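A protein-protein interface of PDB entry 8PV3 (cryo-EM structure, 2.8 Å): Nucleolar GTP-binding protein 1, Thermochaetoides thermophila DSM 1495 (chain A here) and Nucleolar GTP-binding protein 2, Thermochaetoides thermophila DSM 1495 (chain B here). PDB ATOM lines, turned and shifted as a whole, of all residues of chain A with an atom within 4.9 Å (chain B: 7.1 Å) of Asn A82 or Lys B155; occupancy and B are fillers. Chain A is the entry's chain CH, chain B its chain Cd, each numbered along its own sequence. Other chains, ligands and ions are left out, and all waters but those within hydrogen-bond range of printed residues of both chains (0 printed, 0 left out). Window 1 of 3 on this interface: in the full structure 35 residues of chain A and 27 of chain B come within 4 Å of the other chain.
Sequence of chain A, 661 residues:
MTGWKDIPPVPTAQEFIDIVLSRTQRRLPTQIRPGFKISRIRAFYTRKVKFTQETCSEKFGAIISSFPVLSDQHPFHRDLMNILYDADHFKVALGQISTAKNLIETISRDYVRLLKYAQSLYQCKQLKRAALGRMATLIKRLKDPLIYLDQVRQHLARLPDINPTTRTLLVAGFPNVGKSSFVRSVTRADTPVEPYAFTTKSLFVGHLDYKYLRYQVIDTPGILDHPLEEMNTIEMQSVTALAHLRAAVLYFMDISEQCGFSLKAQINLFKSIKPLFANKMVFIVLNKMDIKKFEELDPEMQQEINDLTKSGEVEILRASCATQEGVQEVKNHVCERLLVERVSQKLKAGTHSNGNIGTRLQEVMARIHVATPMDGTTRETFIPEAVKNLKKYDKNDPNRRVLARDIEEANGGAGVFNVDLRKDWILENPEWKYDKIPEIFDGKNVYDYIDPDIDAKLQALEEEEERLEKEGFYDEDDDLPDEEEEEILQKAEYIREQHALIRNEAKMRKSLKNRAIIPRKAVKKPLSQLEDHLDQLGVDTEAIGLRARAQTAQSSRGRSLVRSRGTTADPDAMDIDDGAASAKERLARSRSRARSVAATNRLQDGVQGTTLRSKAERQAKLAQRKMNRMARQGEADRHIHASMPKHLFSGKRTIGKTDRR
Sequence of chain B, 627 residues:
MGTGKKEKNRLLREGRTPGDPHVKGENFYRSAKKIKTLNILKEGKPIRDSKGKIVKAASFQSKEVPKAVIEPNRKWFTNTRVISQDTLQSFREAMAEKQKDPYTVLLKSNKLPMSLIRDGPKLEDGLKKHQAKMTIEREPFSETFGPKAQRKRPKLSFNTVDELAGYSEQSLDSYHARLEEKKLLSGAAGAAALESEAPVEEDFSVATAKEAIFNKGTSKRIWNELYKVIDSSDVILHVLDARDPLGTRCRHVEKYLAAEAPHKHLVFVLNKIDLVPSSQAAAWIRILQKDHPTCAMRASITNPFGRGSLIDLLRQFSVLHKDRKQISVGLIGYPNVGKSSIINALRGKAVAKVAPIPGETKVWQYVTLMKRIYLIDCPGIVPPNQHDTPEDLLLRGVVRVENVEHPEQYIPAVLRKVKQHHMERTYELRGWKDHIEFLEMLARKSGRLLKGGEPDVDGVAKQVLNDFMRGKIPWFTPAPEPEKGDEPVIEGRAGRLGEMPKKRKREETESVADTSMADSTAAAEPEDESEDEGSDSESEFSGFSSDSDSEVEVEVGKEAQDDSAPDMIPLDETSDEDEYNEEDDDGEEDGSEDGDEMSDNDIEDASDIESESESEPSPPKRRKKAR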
ATOM      1  N   ARG A  78       5.597   5.241  20.289  1.00  0.00           N
ATOM      2  CA  ARG A  78       4.614   4.167  20.175  1.00  0.00           C
ATOM      3  C   ARG A  78       4.711   3.463  18.830  1.00  0.00           C
ATOM      4  O   ARG A  78       4.730   2.227  18.765  1.00  0.00           O
ATOM      5  CB  ARG A  78       3.209   4.726  20.379  1.00  0.00           C
ATOM      6  CG  ARG A  78       2.104   3.718  20.153  1.00  0.00           C
ATOM      7  CD  ARG A  78       0.756   4.397  20.185  1.00  0.00           C
ATOM      8  NE  ARG A  78       0.757   5.535  21.094  1.00  0.00           N
ATOM      9  CZ  ARG A  78       0.149   6.687  20.850  1.00  0.00           C
ATOM     10  NH1 ARG A  78      -0.539   6.884  19.738  1.00  0.00           N
ATOM     11  NH2 ARG A  78       0.239   7.669  21.743  1.00  0.00           N
ATOM     12  N   ASP A  79       4.825   4.228  17.746  1.00  0.00           N
ATOM     13  CA  ASP A  79       4.896   3.600  16.434  1.00  0.00           C
ATOM     14  C   ASP A  79       6.261   2.965  16.193  1.00  0.00           C
ATOM     15  O   ASP A  79       6.365   1.974  15.466  1.00  0.00           O
ATOM     16  CB  ASP A  79       4.542   4.620  15.358  1.00  0.00           C
ATOM     17  CG  ASP A  79       3.054   4.899  15.306  1.00  0.00           C
ATOM     18  OD1 ASP A  79       2.268   3.946  15.494  1.00  0.00           O
ATOM     19  OD2 ASP A  79       2.661   6.064  15.112  1.00  0.00           O
ATOM     20  N   LEU A  80       7.315   3.488  16.827  1.00  0.00           N
ATOM     21  CA  LEU A  80       8.624   2.849  16.734  1.00  0.00           C
ATOM     22  C   LEU A  80       8.626   1.494  17.429  1.00  0.00           C
ATOM     23  O   LEU A  80       9.210   0.528  16.924  1.00  0.00           O
ATOM     24  CB  LEU A  80       9.695   3.759  17.328  1.00  0.00           C
ATOM     25  CG  LEU A  80      11.130   3.250  17.217  1.00  0.00           C
ATOM     26  CD1 LEU A  80      11.495   2.999  15.768  1.00  0.00           C
ATOM     27  CD2 LEU A  80      12.086   4.240  17.845  1.00  0.00           C
ATOM     28  N   MET A  81       7.987   1.405  18.599  1.00  0.00           N
ATOM     29  CA  MET A  81       7.848   0.106  19.250  1.00  0.00           C
ATOM     30  C   MET A  81       6.942  -0.818  18.450  1.00  0.00           C
ATOM     31  O   MET A  81       7.153  -2.031  18.439  1.00  0.00           O
ATOM     32  CB  MET A  81       7.332   0.255  20.682  1.00  0.00           C
ATOM     33  CG  MET A  81       8.145   1.189  21.552  1.00  0.00           C
ATOM     34  SD  MET A  81       7.638   1.184  23.277  1.00  0.00           S
ATOM     35  CE  MET A  81       8.973   2.120  24.015  1.00  0.00           C
ATOM     36  N   ASN A  82       5.940  -0.263  17.765  1.00  0.00           N
ATOM     37  CA  ASN A  82       5.093  -1.082  16.899  1.00  0.00           C
ATOM     38  C   ASN A  82       5.865  -1.605  15.687  1.00  0.00           C
ATOM     39  O   ASN A  82       5.524  -2.654  15.128  1.00  0.00           O
ATOM     40  CB  ASN A  82       3.870  -0.277  16.457  1.00  0.00           C
ATOM     41  CG  ASN A  82       3.062  -0.980  15.387  1.00  0.00           C
ATOM     42  OD1 ASN A  82       2.455  -2.019  15.633  1.00  0.00           O
ATOM     43  ND2 ASN A  82       3.060  -0.420  14.184  1.00  0.00           N
ATOM     44  N   ILE A  83       6.883  -0.874  15.241  1.00  0.00           N
ATOM     45  CA  ILE A  83       7.687  -1.365  14.124  1.00  0.00           C
ATOM     46  C   ILE A  83       8.701  -2.400  14.597  1.00  0.00           C
ATOM     47  O   ILE A  83       8.803  -3.493  14.027  1.00  0.00           O
ATOM     48  CB  ILE A  83       8.366  -0.197  13.389  1.00  0.00           C
ATOM     49  CG1 ILE A  83       7.307   0.667  12.711  1.00  0.00           C
ATOM     50  CG2 ILE A  83       9.397  -0.712  12.402  1.00  0.00           C
ATOM     51  CD1 ILE A  83       6.448  -0.088  11.737  1.00  0.00           C
ATOM     52  N   LEU A  84       9.457  -2.078  15.649  1.00  0.00           N
ATOM     53  CA  LEU A  84      10.513  -2.972  16.120  1.00  0.00           C
ATOM     54  C   LEU A  84       9.940  -4.255  16.705  1.00  0.00           C
ATOM     55  O   LEU A  84      10.516  -5.336  16.543  1.00  0.00           O
ATOM     56  CB  LEU A  84      11.363  -2.266  17.173  1.00  0.00           C
ATOM     57  CG  LEU A  84      12.260  -1.113  16.751  1.00  0.00           C
ATOM     58  CD1 LEU A  84      12.762  -0.405  17.985  1.00  0.00           C
ATOM     59  CD2 LEU A  84      13.418  -1.631  15.929  1.00  0.00           C
ATOM     60  N   TYR A  85       8.814  -4.143  17.395  1.00  0.00           N
ATOM     61  CA  TYR A  85       8.213  -5.200  18.188  1.00  0.00           C
ATOM     62  C   TYR A  85       6.812  -5.308  17.617  1.00  0.00           C
ATOM     63  O   TYR A  85       6.273  -4.303  17.160  1.00  0.00           O
ATOM     64  CB  TYR A  85       8.124  -4.770  19.655  1.00  0.00           C
ATOM     65  CG  TYR A  85       9.429  -4.408  20.335  1.00  0.00           C
ATOM     66  CD1 TYR A  85      10.662  -4.826  19.848  1.00  0.00           C
ATOM     67  CD2 TYR A  85       9.423  -3.486  21.367  1.00  0.00           C
ATOM     68  CE1 TYR A  85      11.834  -4.427  20.449  1.00  0.00           C
ATOM     69  CE2 TYR A  85      10.583  -3.075  21.960  1.00  0.00           C
ATOM     70  CZ  TYR A  85      11.785  -3.547  21.501  1.00  0.00           C
ATOM     71  OH  TYR A  85      12.936  -3.126  22.114  1.00  0.00           O
ATOM     72  N   ASP A  86       6.208  -6.483  17.613  1.00  0.00           N
ATOM     73  CA  ASP A  86       4.800  -6.468  17.255  1.00  0.00           C
ATOM     74  C   ASP A  86       4.002  -5.925  18.432  1.00  0.00           C
ATOM     75  O   ASP A  86       4.153  -6.390  19.563  1.00  0.00           O
ATOM     76  CB  ASP A  86       4.314  -7.851  16.850  1.00  0.00           C
ATOM     77  CG  ASP A  86       2.960  -7.814  16.186  1.00  0.00           C
ATOM     78  OD1 ASP A  86       2.870  -7.330  15.041  1.00  0.00           O
ATOM     79  OD2 ASP A  86       1.986  -8.283  16.802  1.00  0.00           O
ATOM     80  N   ALA A  87       3.194  -4.893  18.174  1.00  0.00           N
ATOM     81  CA  ALA A  87       2.422  -4.271  19.247  1.00  0.00           C
ATOM     82  C   ALA A  87       1.384  -5.233  19.805  1.00  0.00           C
ATOM     83  O   ALA A  87       1.161  -5.284  21.023  1.00  0.00           O
ATOM     84  CB  ALA A  87       1.751  -2.995  18.745  1.00  0.00           C
ATOM     85  N   ASP A  88       0.751  -6.014  18.925  1.00  0.00           N
ATOM     86  CA  ASP A  88      -0.196  -7.027  19.369  1.00  0.00           C
ATOM     87  C   ASP A  88       0.491  -8.086  20.218  1.00  0.00           C
ATOM     88  O   ASP A  88      -0.029  -8.478  21.264  1.00  0.00           O
ATOM     89  CB  ASP A  88      -0.879  -7.668  18.163  1.00  0.00           C
ATOM     90  CG  ASP A  88      -1.856  -6.736  17.483  1.00  0.00           C
ATOM     91  OD1 ASP A  88      -2.266  -5.738  18.112  1.00  0.00           O
ATOM     92  OD2 ASP A  88      -2.214  -7.000  16.317  1.00  0.00           O
ATOM     93  N   GLU B 139       0.964 -15.962  14.250  1.00  0.00           N
ATOM     94  CA  GLU B 139       2.357 -15.533  14.335  1.00  0.00           C
ATOM     95  C   GLU B 139       2.858 -15.839  15.740  1.00  0.00           C
ATOM     96  O   GLU B 139       2.482 -15.141  16.697  1.00  0.00           O
ATOM     97  CB  GLU B 139       2.489 -14.047  14.026  1.00  0.00           C
ATOM     98  CG  GLU B 139       2.112 -13.666  12.604  1.00  0.00           C
ATOM     99  CD  GLU B 139       2.124 -12.168  12.376  1.00  0.00           C
ATOM    100  OE1 GLU B 139       2.303 -11.417  13.355  1.00  0.00           O
ATOM    101  OE2 GLU B 139       1.944 -11.742  11.216  1.00  0.00           O
ATOM    102  N   ARG B 151       9.987 -12.361  11.094  1.00  0.00           N
ATOM    103  CA  ARG B 151       9.103 -11.273  10.706  1.00  0.00           C
ATOM    104  C   ARG B 151       9.870 -10.196   9.951  1.00  0.00           C
ATOM    105  O   ARG B 151      10.924  -9.735  10.395  1.00  0.00           O
ATOM    106  CB  ARG B 151       8.438 -10.680  11.948  1.00  0.00           C
ATOM    107  CG  ARG B 151       7.866  -9.288  11.766  1.00  0.00           C
ATOM    108  CD  ARG B 151       7.144  -8.833  13.021  1.00  0.00           C
ATOM    109  NE  ARG B 151       6.737  -7.437  12.951  1.00  0.00           N
ATOM    110  CZ  ARG B 151       7.374  -6.443  13.554  1.00  0.00           C
ATOM    111  NH1 ARG B 151       8.460  -6.656  14.274  1.00  0.00           N
ATOM    112  NH2 ARG B 151       6.907  -5.205  13.431  1.00  0.00           N
ATOM    113  N   ARG B 153       7.694  -7.917   7.441  1.00  0.00           N
ATOM    114  CA  ARG B 153       6.644  -6.934   7.201  1.00  0.00           C
ATOM    115  C   ARG B 153       5.950  -6.585   8.505  1.00  0.00           C
ATOM    116  O   ARG B 153       5.437  -7.485   9.183  1.00  0.00           O
ATOM    117  CB  ARG B 153       5.614  -7.475   6.213  1.00  0.00           C
ATOM    118  CG  ARG B 153       6.125  -7.714   4.809  1.00  0.00           C
ATOM    119  CD  ARG B 153       6.494  -6.414   4.128  1.00  0.00           C
ATOM    120  NE  ARG B 153       7.062  -6.641   2.805  1.00  0.00           N
ATOM    121  CZ  ARG B 153       8.334  -6.934   2.575  1.00  0.00           C
ATOM    122  NH1 ARG B 153       9.210  -7.040   3.560  1.00  0.00           N
ATOM    123  NH2 ARG B 153       8.740  -7.121   1.322  1.00  0.00           N
ATOM    124  N   PRO B 154       5.904  -5.319   8.895  1.00  0.00           N
ATOM    125  CA  PRO B 154       5.140  -4.933  10.083  1.00  0.00           C
ATOM    126  C   PRO B 154       3.650  -4.856   9.776  1.00  0.00           C
ATOM    127  O   PRO B 154       3.215  -4.908   8.627  1.00  0.00           O
ATOM    128  CB  PRO B 154       5.704  -3.555  10.426  1.00  0.00           C
ATOM    129  CG  PRO B 154       6.113  -3.011   9.123  1.00  0.00           C
ATOM    130  CD  PRO B 154       6.603  -4.168   8.300  1.00  0.00           C
ATOM    131  N   LYS B 155       2.868  -4.725  10.842  1.00  0.00           N
ATOM    132  CA  LYS B 155       1.425  -4.543  10.745  1.00  0.00           C
ATOM    133  C   LYS B 155       1.134  -3.055  10.888  1.00  0.00           C
ATOM    134  O   LYS B 155       1.386  -2.469  11.946  1.00  0.00           O
ATOM    135  CB  LYS B 155       0.704  -5.373  11.812  1.00  0.00           C
ATOM    136  CG  LYS B 155      -0.830  -5.306  11.824  1.00  0.00           C
ATOM    137  CD  LYS B 155      -1.385  -4.253  12.782  1.00  0.00           C
ATOM    138  CE  LYS B 155      -1.176  -4.654  14.234  1.00  0.00           C
ATOM    139  NZ  LYS B 155      -1.722  -3.643  15.184  1.00  0.00           N
ATOM    140  N   LEU B 156       0.604  -2.451   9.831  1.00  0.00           N
ATOM    141  CA  LEU B 156       0.372  -1.017   9.783  1.00  0.00           C
ATOM    142  C   LEU B 156      -1.121  -0.722   9.735  1.00  0.00           C
ATOM    143  O   LEU B 156      -1.902  -1.442   9.108  1.00  0.00           O
ATOM    144  CB  LEU B 156       1.064  -0.389   8.568  1.00  0.00           C
ATOM    145  CG  LEU B 156       2.567  -0.621   8.412  1.00  0.00           C
ATOM    146  CD1 LEU B 156       3.048  -0.074   7.084  1.00  0.00           C
ATOM    147  CD2 LEU B 156       3.333   0.011   9.556  1.00  0.00           C
ATOM    148  N   SER B 157      -1.507   0.357  10.412  1.00  0.00           N
ATOM    149  CA  SER B 157      -2.878   0.844  10.404  1.00  0.00           C
ATOM    150  C   SER B 157      -3.135   1.817   9.263  1.00  0.00           C
ATOM    151  O   SER B 157      -4.207   2.427   9.207  1.00  0.00           O
ATOM    152  CB  SER B 157      -3.206   1.504  11.743  1.00  0.00           C
ATOM    153  OG  SER B 157      -2.151   2.350  12.157  1.00  0.00           O
ATOM    154  N   PHE B 158      -2.172   1.976   8.360  1.00  0.00           N
ATOM    155  CA  PHE B 158      -2.290   2.868   7.219  1.00  0.00           C
ATOM    156  C   PHE B 158      -1.739   2.156   5.994  1.00  0.00           C
ATOM    157  O   PHE B 158      -0.924   1.238   6.101  1.00  0.00           O
ATOM    158  CB  PHE B 158      -1.543   4.189   7.453  1.00  0.00           C
ATOM    159  CG  PHE B 158      -0.162   4.015   8.020  1.00  0.00           C
ATOM    160  CD1 PHE B 158       0.926   3.823   7.185  1.00  0.00           C
ATOM    161  CD2 PHE B 158       0.052   4.052   9.388  1.00  0.00           C
ATOM    162  CE1 PHE B 158       2.194   3.664   7.701  1.00  0.00           C
ATOM    163  CE2 PHE B 158       1.319   3.890   9.909  1.00  0.00           C
ATOM    164  CZ  PHE B 158       2.391   3.695   9.065  1.00  0.00           C
ATOM    165  N   TYR B 167      -2.848  10.211   9.858  1.00  0.00           N
ATOM    166  CA  TYR B 167      -2.850   9.408  11.074  1.00  0.00           C
ATOM    167  C   TYR B 167      -1.855   9.938  12.092  1.00  0.00           C
ATOM    168  O   TYR B 167      -2.137   9.935  13.294  1.00  0.00           O
ATOM    169  CB  TYR B 167      -2.556   7.945  10.726  1.00  0.00           C
ATOM    170  CG  TYR B 167      -2.038   7.095  11.869  1.00  0.00           C
ATOM    171  CD1 TYR B 167      -2.915   6.480  12.752  1.00  0.00           C
ATOM    172  CD2 TYR B 167      -0.674   6.861  12.030  1.00  0.00           C
ATOM    173  CE1 TYR B 167      -2.451   5.695  13.786  1.00  0.00           C
ATOM    174  CE2 TYR B 167      -0.203   6.079  13.064  1.00  0.00           C
ATOM    175  CZ  TYR B 167      -1.096   5.496  13.936  1.00  0.00           C
ATOM    176  OH  TYR B 167      -0.631   4.712  14.964  1.00  0.00           O
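The side-chain hydroxyl (OH) of Tyr B167 is in hydrogen-bond range of the side-chain carboxylate (OD1) of Asp A79, at 3.0 Å. The guanidinium group of Arg B151 is in hydrogen-bond range of the backbone carbonyl oxygen of Asn A82 (3.4 Å). The guanidinium group (NH1) of Arg B151 is in hydrogen-bond range of the backbone carbonyl oxygen (O) of Leu A84. The backbone carbonyl oxygen (O) of Lys B155 sits at hydrogen-bond distance from the side-chain amide nitrogen (ND2) of Asn A82 (3.5 Å). NZ of Lys B155 is in salt-bridge range of OD2 of Asp A88 (3.6 Å). The backbone carbonyl oxygen (O) of Ile A83 is in hydrogen-bond range of the guanidinium group (NH2) of Arg B151 (2.6 Å).
The side-chain carboxylate (OD2) of Asp A86 sits close to the backbone NH (N) of Asp A88, 3.3 Å away.
Among the printed residues, pairs that only touch across the chains: Ile A83 with Pro B154 (3.8 Å), Ile A83 with Leu B156 (3.8 Å) and Tyr A85 with Arg B151 (3.9 Å).
Arg A78 touches none of the printed residues of chain B. Asn A82 touches just these residues of chain B: Arg B151 (3.4 Å) and Lys B155 (3.5 Å). Printed residues of chain B within 4 Å of Ile A83: Arg B151 (2.6 Å), Pro B154 (3.8 Å) and Leu B156 (3.8 Å). Of the printed residues of chain B, Leu A84 touches Arg B151 (3.3 Å). Of the printed residues of chain A, Arg B151 touches Asn A82 (3.4 Å), Ile A83 (2.6 Å), Leu A84 (3.3 Å) and Tyr A85 (3.9 Å). Of the printed residues of chain A, Tyr B167 touches Asp A79. The nearest residue of chain B that does not touch Asn A82 is Leu B156 (4.7 Å). The nearest printed residue of chain A that does not touch Tyr B167 is Arg A78 (5.2 Å).
Hydrophobic or aromatic side chains of chain B within 4 Å of the printed part of chain A: Pro B154, Leu B156 and Tyr B167. Of the 11 printed residues of chain A, 6 touch a printed residue of chain B. Hydrophobic or aromatic side chains of chain A within 4 Å of the printed part of chain B: Ile A83. Along chain A the printed residues that touch a printed residue of chain B span positions 79 to 88. Among the printed residues, 9 pairs touch across the chains.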
